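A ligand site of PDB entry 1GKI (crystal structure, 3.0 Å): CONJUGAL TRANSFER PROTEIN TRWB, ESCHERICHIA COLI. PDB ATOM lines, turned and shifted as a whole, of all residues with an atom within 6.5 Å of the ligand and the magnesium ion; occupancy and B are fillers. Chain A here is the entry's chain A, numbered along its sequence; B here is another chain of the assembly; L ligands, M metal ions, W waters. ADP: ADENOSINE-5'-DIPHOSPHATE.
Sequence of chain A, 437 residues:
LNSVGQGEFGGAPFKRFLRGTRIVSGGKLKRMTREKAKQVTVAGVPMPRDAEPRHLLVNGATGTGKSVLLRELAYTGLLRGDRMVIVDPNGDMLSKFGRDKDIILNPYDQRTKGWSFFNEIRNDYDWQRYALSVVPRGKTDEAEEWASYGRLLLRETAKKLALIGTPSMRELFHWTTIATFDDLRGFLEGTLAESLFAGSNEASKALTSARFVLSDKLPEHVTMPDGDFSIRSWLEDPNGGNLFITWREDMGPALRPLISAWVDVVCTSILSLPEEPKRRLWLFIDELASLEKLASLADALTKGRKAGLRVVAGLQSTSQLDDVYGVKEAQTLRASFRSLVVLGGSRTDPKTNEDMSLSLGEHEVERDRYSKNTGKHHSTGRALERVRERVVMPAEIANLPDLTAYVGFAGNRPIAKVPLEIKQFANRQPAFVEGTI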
ATOM      1  N   GLY A  60       2.868  16.116   9.341  1.00  0.00           N
ATOM      2  CA  GLY A  60       3.922  16.670   8.506  1.00  0.00           C
ATOM      3  C   GLY A  60       5.257  16.896   9.189  1.00  0.00           C
ATOM      4  O   GLY A  60       5.321  17.283  10.354  1.00  0.00           O
ATOM      5  N   ALA A  61       6.336  16.679   8.448  1.00  0.00           N
ATOM      6  CA  ALA A  61       7.680  16.863   8.990  1.00  0.00           C
ATOM      7  C   ALA A  61       7.857  18.274   9.501  1.00  0.00           C
ATOM      8  O   ALA A  61       7.116  19.170   9.146  1.00  0.00           O
ATOM      9  CB  ALA A  61       8.710  16.565   7.905  1.00  0.00           C
ATOM     10  N   THR A  62       8.858  18.466  10.357  1.00  0.00           N
ATOM     11  CA  THR A  62       9.125  19.782  10.906  1.00  0.00           C
ATOM     12  C   THR A  62       9.487  20.752   9.795  1.00  0.00           C
ATOM     13  O   THR A  62      10.335  20.451   8.942  1.00  0.00           O
ATOM     14  CB  THR A  62      10.265  19.710  11.959  1.00  0.00           C
ATOM     15  OG1 THR A  62      10.600  21.036  12.410  1.00  0.00           O
ATOM     16  CG2 THR A  62      11.516  19.052  11.373  1.00  0.00           C
ATOM     17  N   GLY A  63       8.807  21.897   9.779  1.00  0.00           N
ATOM     18  CA  GLY A  63       9.082  22.919   8.776  1.00  0.00           C
ATOM     19  C   GLY A  63       8.405  22.771   7.427  1.00  0.00           C
ATOM     20  O   GLY A  63       8.845  23.357   6.448  1.00  0.00           O
ATOM     21  N   THR A  64       7.319  22.007   7.386  1.00  0.00           N
ATOM     22  CA  THR A  64       6.597  21.783   6.139  1.00  0.00           C
ATOM     23  C   THR A  64       5.333  22.635   5.998  1.00  0.00           C
ATOM     24  O   THR A  64       4.800  22.759   4.899  1.00  0.00           O
ATOM     25  CB  THR A  64       6.217  20.293   5.966  1.00  0.00           C
ATOM     26  OG1 THR A  64       5.364  19.896   7.057  1.00  0.00           O
ATOM     27  CG2 THR A  64       7.458  19.417   5.951  1.00  0.00           C
ATOM     28  N   GLY A  65       4.844  23.197   7.086  1.00  0.00           N
ATOM     29  CA  GLY A  65       3.659  24.040   6.978  1.00  0.00           C
ATOM     30  C   GLY A  65       2.465  23.757   7.874  1.00  0.00           C
ATOM     31  O   GLY A  65       1.396  24.358   7.683  1.00  0.00           O
ATOM     32  N   LYS A  66       2.604  22.858   8.845  1.00  0.00           N
ATOM     33  CA  LYS A  66       1.491  22.548   9.726  1.00  0.00           C
ATOM     34  C   LYS A  66       0.947  23.842  10.335  1.00  0.00           C
ATOM     35  O   LYS A  66      -0.262  24.100  10.330  1.00  0.00           O
ATOM     36  CB  LYS A  66       1.942  21.614  10.862  1.00  0.00           C
ATOM     37  CG  LYS A  66       2.259  20.201  10.419  1.00  0.00           C
ATOM     38  CD  LYS A  66       2.621  19.307  11.602  1.00  0.00           C
ATOM     39  CE  LYS A  66       3.860  19.795  12.324  1.00  0.00           C
ATOM     40  NZ  LYS A  66       5.008  19.972  11.397  1.00  0.00           N
ATOM     41  N   SER A  67       1.857  24.677  10.832  1.00  0.00           N
ATOM     42  CA  SER A  67       1.472  25.936  11.459  1.00  0.00           C
ATOM     43  C   SER A  67       0.794  26.877  10.482  1.00  0.00           C
ATOM     44  O   SER A  67      -0.175  27.551  10.851  1.00  0.00           O
ATOM     45  CB  SER A  67       2.701  26.608  12.061  1.00  0.00           C
ATOM     46  OG  SER A  67       3.293  25.765  13.047  1.00  0.00           O
ATOM     47  N   VAL A  68       1.291  26.952   9.256  1.00  0.00           N
ATOM     48  CA  VAL A  68       0.681  27.810   8.249  1.00  0.00           C
ATOM     49  C   VAL A  68      -0.739  27.314   8.050  1.00  0.00           C
ATOM     50  O   VAL A  68      -1.702  28.099   8.110  1.00  0.00           O
ATOM     51  CB  VAL A  68       1.436  27.755   6.886  1.00  0.00           C
ATOM     52  CG1 VAL A  68       0.550  28.297   5.767  1.00  0.00           C
ATOM     53  CG2 VAL A  68       2.711  28.584   6.953  1.00  0.00           C
ATOM     54  N   LEU A  69      -0.879  26.015   7.845  1.00  0.00           N
ATOM     55  CA  LEU A  69      -2.184  25.420   7.607  1.00  0.00           C
ATOM     56  C   LEU A  69      -3.171  25.653   8.731  1.00  0.00           C
ATOM     57  O   LEU A  69      -4.323  26.028   8.472  1.00  0.00           O
ATOM     58  CB  LEU A  69      -2.036  23.916   7.343  1.00  0.00           C
ATOM     59  CG  LEU A  69      -3.269  23.230   6.784  1.00  0.00           C
ATOM     60  CD1 LEU A  69      -2.859  21.941   6.120  1.00  0.00           C
ATOM     61  CD2 LEU A  69      -4.287  22.979   7.869  1.00  0.00           C
ATOM     62  N   ARG A  71      -3.047  28.015  11.034  1.00  0.00           N
ATOM     63  CA  ARG A  71      -3.293  29.434  11.170  1.00  0.00           C
ATOM     64  C   ARG A  71      -4.365  29.860  10.160  1.00  0.00           C
ATOM     65  O   ARG A  71      -5.273  30.620  10.506  1.00  0.00           O
ATOM     66  CB  ARG A  71      -1.997  30.215  10.939  1.00  0.00           C
ATOM     67  CG  ARG A  71      -1.924  31.525  11.713  1.00  0.00           C
ATOM     68  CD  ARG A  71      -0.625  32.267  11.433  1.00  0.00           C
ATOM     69  NE  ARG A  71       0.534  31.432  11.702  1.00  0.00           N
ATOM     70  CZ  ARG A  71       1.542  31.274  10.845  1.00  0.00           C
ATOM     71  NH1 ARG A  71       1.535  31.891   9.667  1.00  0.00           N
ATOM     72  NH2 ARG A  71       2.552  30.482  11.185  1.00  0.00           N
ATOM     73  N   LYS A  96      -1.894  37.603  16.475  1.00  0.00           N
ATOM     74  CA  LYS A  96      -2.503  37.832  15.171  1.00  0.00           C
ATOM     75  C   LYS A  96      -4.007  37.993  15.190  1.00  0.00           C
ATOM     76  O   LYS A  96      -4.533  38.908  14.556  1.00  0.00           O
ATOM     77  CB  LYS A  96      -2.160  36.690  14.209  1.00  0.00           C
ATOM     78  CG  LYS A  96      -0.695  36.319  14.127  1.00  0.00           C
ATOM     79  CD  LYS A  96       0.142  37.317  13.332  1.00  0.00           C
ATOM     80  CE  LYS A  96       1.566  36.794  13.181  1.00  0.00           C
ATOM     81  NZ  LYS A  96       1.564  35.376  12.690  1.00  0.00           N
ATOM     82  N   ASP A 286      -1.629  22.554  18.274  1.00  0.00           N
ATOM     83  CA  ASP A 286      -0.495  22.606  17.358  1.00  0.00           C
ATOM     84  C   ASP A 286       0.271  21.291  17.283  1.00  0.00           C
ATOM     85  O   ASP A 286       0.591  20.814  16.202  1.00  0.00           O
ATOM     86  CB  ASP A 286       0.467  23.724  17.772  1.00  0.00           C
ATOM     87  CG  ASP A 286       1.275  23.355  18.998  1.00  0.00           C
ATOM     88  OD1 ASP A 286       2.521  23.427  18.931  1.00  0.00           O
ATOM     89  OD2 ASP A 286       0.660  22.998  20.035  1.00  0.00           O
ATOM     90  N   GLU A 287       0.560  20.699  18.431  1.00  0.00           N
ATOM     91  CA  GLU A 287       1.282  19.448  18.445  1.00  0.00           C
ATOM     92  C   GLU A 287       0.719  18.473  19.473  1.00  0.00           C
ATOM     93  O   GLU A 287       1.048  18.524  20.652  1.00  0.00           O
ATOM     94  CB  GLU A 287       2.771  19.696  18.720  1.00  0.00           C
ATOM     95  CG  GLU A 287       3.612  18.445  18.546  1.00  0.00           C
ATOM     96  CD  GLU A 287       3.424  17.825  17.160  1.00  0.00           C
ATOM     97  OE1 GLU A 287       3.122  16.606  17.093  1.00  0.00           O
ATOM     98  OE2 GLU A 287       3.586  18.562  16.156  1.00  0.00           O
ATOM     99  N   GLN A 316       3.877  15.287  14.014  1.00  0.00           N
ATOM    100  CA  GLN A 316       5.067  15.103  13.190  1.00  0.00           C
ATOM    101  C   GLN A 316       5.320  13.639  12.889  1.00  0.00           C
ATOM    102  O   GLN A 316       5.257  13.216  11.732  1.00  0.00           O
ATOM    103  CB  GLN A 316       6.287  15.708  13.859  1.00  0.00           C
ATOM    104  CG  GLN A 316       6.267  17.218  13.848  1.00  0.00           C
ATOM    105  CD  GLN A 316       7.444  17.819  14.573  1.00  0.00           C
ATOM    106  OE1 GLN A 316       8.180  18.649  14.034  1.00  0.00           O
ATOM    107  NE2 GLN A 316       7.630  17.400  15.825  1.00  0.00           N
ATOM    108  N   LEU A 343       1.601  16.456   4.822  1.00  0.00           N
ATOM    109  CA  LEU A 343       2.557  17.454   4.365  1.00  0.00           C
ATOM    110  C   LEU A 343       3.943  16.963   3.951  1.00  0.00           C
ATOM    111  O   LEU A 343       4.850  17.764   3.741  1.00  0.00           O
ATOM    112  CB  LEU A 343       2.716  18.525   5.448  1.00  0.00           C
ATOM    113  CG  LEU A 343       1.616  19.578   5.512  1.00  0.00           C
ATOM    114  CD1 LEU A 343       1.713  20.372   6.799  1.00  0.00           C
ATOM    115  CD2 LEU A 343       1.751  20.497   4.319  1.00  0.00           C
ATOM    116  N   ASP A 402       8.367  21.840   0.894  1.00  0.00           N
ATOM    117  CA  ASP A 402       7.575  22.412   1.969  1.00  0.00           C
ATOM    118  C   ASP A 402       6.345  23.147   1.400  1.00  0.00           C
ATOM    119  O   ASP A 402       6.265  23.425   0.202  1.00  0.00           O
ATOM    120  CB  ASP A 402       8.412  23.371   2.825  1.00  0.00           C
ATOM    121  CG  ASP A 402       9.653  22.701   3.422  1.00  0.00           C
ATOM    122  OD1 ASP A 402       9.540  21.606   4.020  1.00  0.00           O
ATOM    123  OD2 ASP A 402      10.757  23.283   3.320  1.00  0.00           O
ATOM    124  N   LEU A 403       5.373  23.437   2.261  1.00  0.00           N
ATOM    125  CA  LEU A 403       4.160  24.126   1.858  1.00  0.00           C
ATOM    126  C   LEU A 403       3.375  23.439   0.732  1.00  0.00           C
ATOM    127  O   LEU A 403       2.721  24.093  -0.072  1.00  0.00           O
ATOM    128  CB  LEU A 403       4.497  25.569   1.463  1.00  0.00           C
ATOM    129  CG  LEU A 403       5.064  26.387   2.620  1.00  0.00           C
ATOM    130  CD1 LEU A 403       5.562  27.706   2.115  1.00  0.00           C
ATOM    131  CD2 LEU A 403       3.982  26.575   3.659  1.00  0.00           C
ATOM    132  N   ILE A 422       1.479  31.034   2.026  1.00  0.00           N
ATOM    133  CA  ILE A 422       1.828  31.686   3.277  1.00  0.00           C
ATOM    134  C   ILE A 422       1.161  33.058   3.371  1.00  0.00           C
ATOM    135  O   ILE A 422       1.696  34.038   2.852  1.00  0.00           O
ATOM    136  CB  ILE A 422       3.344  31.911   3.401  1.00  0.00           C
ATOM    137  CG1 ILE A 422       4.084  30.593   3.299  1.00  0.00           C
ATOM    138  CG2 ILE A 422       3.667  32.604   4.724  1.00  0.00           C
ATOM    139  CD1 ILE A 422       5.600  30.739   3.331  1.00  0.00           C
ATOM    140  N   LYS A 423       0.007  33.125   4.013  1.00  0.00           N
ATOM    141  CA  LYS A 423      -0.681  34.402   4.139  1.00  0.00           C
ATOM    142  C   LYS A 423      -0.055  35.224   5.284  1.00  0.00           C
ATOM    143  O   LYS A 423       0.406  34.666   6.280  1.00  0.00           O
ATOM    144  CB  LYS A 423      -2.186  34.202   4.398  1.00  0.00           C
ATOM    145  CG  LYS A 423      -2.997  35.471   4.183  1.00  0.00           C
ATOM    146  CD  LYS A 423      -4.504  35.268   4.394  1.00  0.00           C
ATOM    147  CE  LYS A 423      -5.287  36.469   3.871  1.00  0.00           C
ATOM    148  NZ  LYS A 423      -4.765  37.752   4.425  1.00  0.00           N
ATOM    149  N   GLN A 424      -0.013  36.543   5.108  1.00  0.00           N
ATOM    150  CA  GLN A 424       0.552  37.440   6.111  1.00  0.00           C
ATOM    151  C   GLN A 424      -0.524  38.047   6.991  1.00  0.00           C
ATOM    152  O   GLN A 424      -1.551  38.540   6.494  1.00  0.00           O
ATOM    153  CB  GLN A 424       1.340  38.555   5.421  1.00  0.00           C
ATOM    154  CG  GLN A 424       2.600  38.080   4.726  1.00  0.00           C
ATOM    155  CD  GLN A 424       3.631  37.511   5.703  1.00  0.00           C
ATOM    156  OE1 GLN A 424       4.724  37.117   5.307  1.00  0.00           O
ATOM    157  NE2 GLN A 424       3.270  37.477   6.981  1.00  0.00           N
ATOM    158  N   ARG B  54      17.298  22.550   8.741  1.00  0.00           N
ATOM    159  CA  ARG B  54      16.447  21.359   8.720  1.00  0.00           C
ATOM    160  C   ARG B  54      17.307  20.189   9.199  1.00  0.00           C
ATOM    161  O   ARG B  54      16.824  19.071   9.356  1.00  0.00           O
ATOM    162  CB  ARG B  54      15.954  21.046   7.315  1.00  0.00           C
ATOM    163  CG  ARG B  54      15.285  22.207   6.596  1.00  0.00           C
ATOM    164  CD  ARG B  54      13.771  22.148   6.636  1.00  0.00           C
ATOM    165  NE  ARG B  54      13.262  23.376   7.199  1.00  0.00           N
ATOM    166  CZ  ARG B  54      12.486  24.284   6.604  1.00  0.00           C
ATOM    167  NH1 ARG B  54      12.126  25.367   7.280  1.00  0.00           N
ATOM    168  NH2 ARG B  54      12.035  24.107   5.371  1.00  0.00           N
ATOM    169  N   THR B 302      13.538  20.715  16.554  1.00  0.00           N
ATOM    170  CA  THR B 302      12.209  21.116  16.102  1.00  0.00           C
ATOM    171  C   THR B 302      11.848  22.595  16.261  1.00  0.00           C
ATOM    172  O   THR B 302      11.067  23.139  15.484  1.00  0.00           O
ATOM    173  CB  THR B 302      11.136  20.257  16.802  1.00  0.00           C
ATOM    174  OG1 THR B 302      10.913  19.070  16.039  1.00  0.00           O
ATOM    175  CG2 THR B 302       9.830  21.029  16.952  1.00  0.00           C
ATOM    176  N   ARG B 305      14.752  26.657  14.687  1.00  0.00           N
ATOM    177  CA  ARG B 305      14.826  27.442  13.463  1.00  0.00           C
ATOM    178  C   ARG B 305      14.940  28.930  13.737  1.00  0.00           C
ATOM    179  O   ARG B 305      15.767  29.615  13.126  1.00  0.00           O
ATOM    180  CB  ARG B 305      13.614  27.163  12.576  1.00  0.00           C
ATOM    181  CG  ARG B 305      13.912  27.237  11.069  1.00  0.00           C
ATOM    182  CD  ARG B 305      12.662  27.246  10.212  1.00  0.00           C
ATOM    183  NE  ARG B 305      11.822  26.060  10.349  1.00  0.00           N
ATOM    184  CZ  ARG B 305      10.528  26.096  10.636  1.00  0.00           C
ATOM    185  NH1 ARG B 305       9.909  27.199  10.825  1.00  0.00           N
ATOM    186  NH2 ARG B 305       9.794  25.041  10.736  1.00  0.00           N
HETATM  187  PB  ADP L   1       5.640  23.307  10.728  1.00  0.00           P
HETATM  188  O1B ADP L   1       6.895  23.785  11.457  1.00  0.00           O
HETATM  189  O2B ADP L   1       5.841  22.163   9.798  1.00  0.00           O
HETATM  190  O3B ADP L   1       4.470  23.053  11.735  1.00  0.00           O
HETATM  191  PA  ADP L   1       5.499  26.037   9.778  1.00  0.00           P
HETATM  192  O1A ADP L   1       5.691  26.554  11.163  1.00  0.00           O
HETATM  193  O2A ADP L   1       4.572  26.734   8.867  1.00  0.00           O
HETATM  194  O3A ADP L   1       5.056  24.483   9.908  1.00  0.00           O
HETATM  195  O5' ADP L   1       6.943  25.940   9.126  1.00  0.00           O
HETATM  196  C5' ADP L   1       7.038  25.469   7.775  1.00  0.00           C
HETATM  197  C4' ADP L   1       7.595  26.451   6.767  1.00  0.00           C
HETATM  198  O4' ADP L   1       6.572  27.472   6.464  1.00  0.00           O
HETATM  199  C3' ADP L   1       8.816  27.295   7.155  1.00  0.00           C
HETATM  200  O3' ADP L   1      10.008  26.531   6.917  1.00  0.00           O
HETATM  201  C2' ADP L   1       8.728  28.517   6.178  1.00  0.00           C
HETATM  202  O2' ADP L   1       9.318  28.185   4.878  1.00  0.00           O
HETATM  203  C1' ADP L   1       7.211  28.701   6.052  1.00  0.00           C
HETATM  204  N9  ADP L   1       6.656  29.891   6.862  1.00  0.00           N
HETATM  205  C8  ADP L   1       5.767  29.872   7.857  1.00  0.00           C
HETATM  206  N7  ADP L   1       5.502  31.042   8.320  1.00  0.00           N
HETATM  207  C5  ADP L   1       6.289  31.907   7.570  1.00  0.00           C
HETATM  208  C6  ADP L   1       6.479  33.366   7.535  1.00  0.00           C
HETATM  209  N6  ADP L   1       5.817  34.208   8.386  1.00  0.00           N
HETATM  210  N1  ADP L   1       7.369  33.869   6.644  1.00  0.00           N
HETATM  211  C2  ADP L   1       8.016  33.052   5.800  1.00  0.00           C
HETATM  212  N3  ADP L   1       7.918  31.701   5.752  1.00  0.00           N
HETATM  213  C4  ADP L   1       7.020  31.189   6.649  1.00  0.00           C
HETATM  214 MG    MG M   1       4.707  23.807  13.752  1.00  0.00          MG
HETATM  215  O   HOH W   1       9.009  33.534   9.702  1.00  0.00           O
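An oxygen (O3') of the ligand lies within hydrogen-bond range of the guanidinium group (NH1) of Arg 54 of chain B, at 2.4 Å. The backbone NH (N) of Ser 67 sits at hydrogen-bond distance from an oxygen (O3A) of the ligand (3.3 Å). N of Thr 64 lies within hydrogen-bond range of O2B of the ligand, at 2.8 Å. The backbone NH (N) of Lys 66 lies within hydrogen-bond range of an oxygen (O3A) of the ligand (3.1 Å). The side-chain amino group of Lys 66 is in salt-bridge range of an oxygen (O2B) of the ligand (2.8 Å). An oxygen (O2B) of the ligand is in hydrogen-bond range of the backbone NH (N) of Gly 63 (3.0 Å). The backbone carbonyl oxygen (O) of Gly 63 sits close to an oxygen (O3') of the ligand. N of Gly 65 is in hydrogen-bond range of O2B of the ligand (3.1 Å). An oxygen (O1B) of the ligand lies within salt-bridge range of the guanidinium group (NH2) of Arg 305 of chain B (3.2 Å). An oxygen (O2A) of the ligand sits close to the backbone NH (N) of Val 68 (3.3 Å).
The guanidinium group of Arg 54 of chain B lies within hydrogen-bond range of the backbone carbonyl oxygen of Gly 63 (3.4 Å). The side-chain carboxylate (OD2) of Asp 402 lies within salt-bridge range of the guanidinium group (NH2) of Arg 54 of chain B (2.6 Å). The side-chain hydroxyl (OG1) of Thr 64 sits at hydrogen-bond distance from the backbone carbonyl oxygen (O) of Ala 61 (2.8 Å). The backbone NH (N) of Leu 403 lies within hydrogen-bond range of the backbone carbonyl oxygen (O) of Thr 64, 2.8 Å away. The side-chain amino group (NZ) of Lys 66 is in hydrogen-bond range of the backbone carbonyl oxygen (O) of Ala 61, 3.2 Å away. The side-chain amino group of Lys 66 lies within hydrogen-bond range of the backbone carbonyl oxygen of Gly 60 (2.9 Å).
The backbone carbonyl oxygen (O) of Ala 61 sits close to an oxygen (O2B) of the ligand (3.3 Å). C of Thr 62 touches O2B of the ligand (3.9 Å). Leu 403 touches the ligand. CD1 of Ile 422 touches N3 of the ligand, 3.5 Å away. Hydrophobic or aromatic side chains within 4 Å of the ligand: Val 68, Leu 403 and Ile 422. 12 residues have an atom within 4 Å of the ligand: Ala 61, Thr 62, Gly 63, Thr 64, Gly 65, Lys 66, Ser 67, Val 68, Leu 403, Ile 422, Arg 54 of chain B and Arg 305 of chain B. The nearest printed residue that does not touch the ligand is Arg 71 (4.2 Å).
The magnesium ion is bound by an oxygen (O3B) of the ligand and the side-chain hydroxyl of Ser 67. The magnesium ion has two donor atoms within binding distance.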
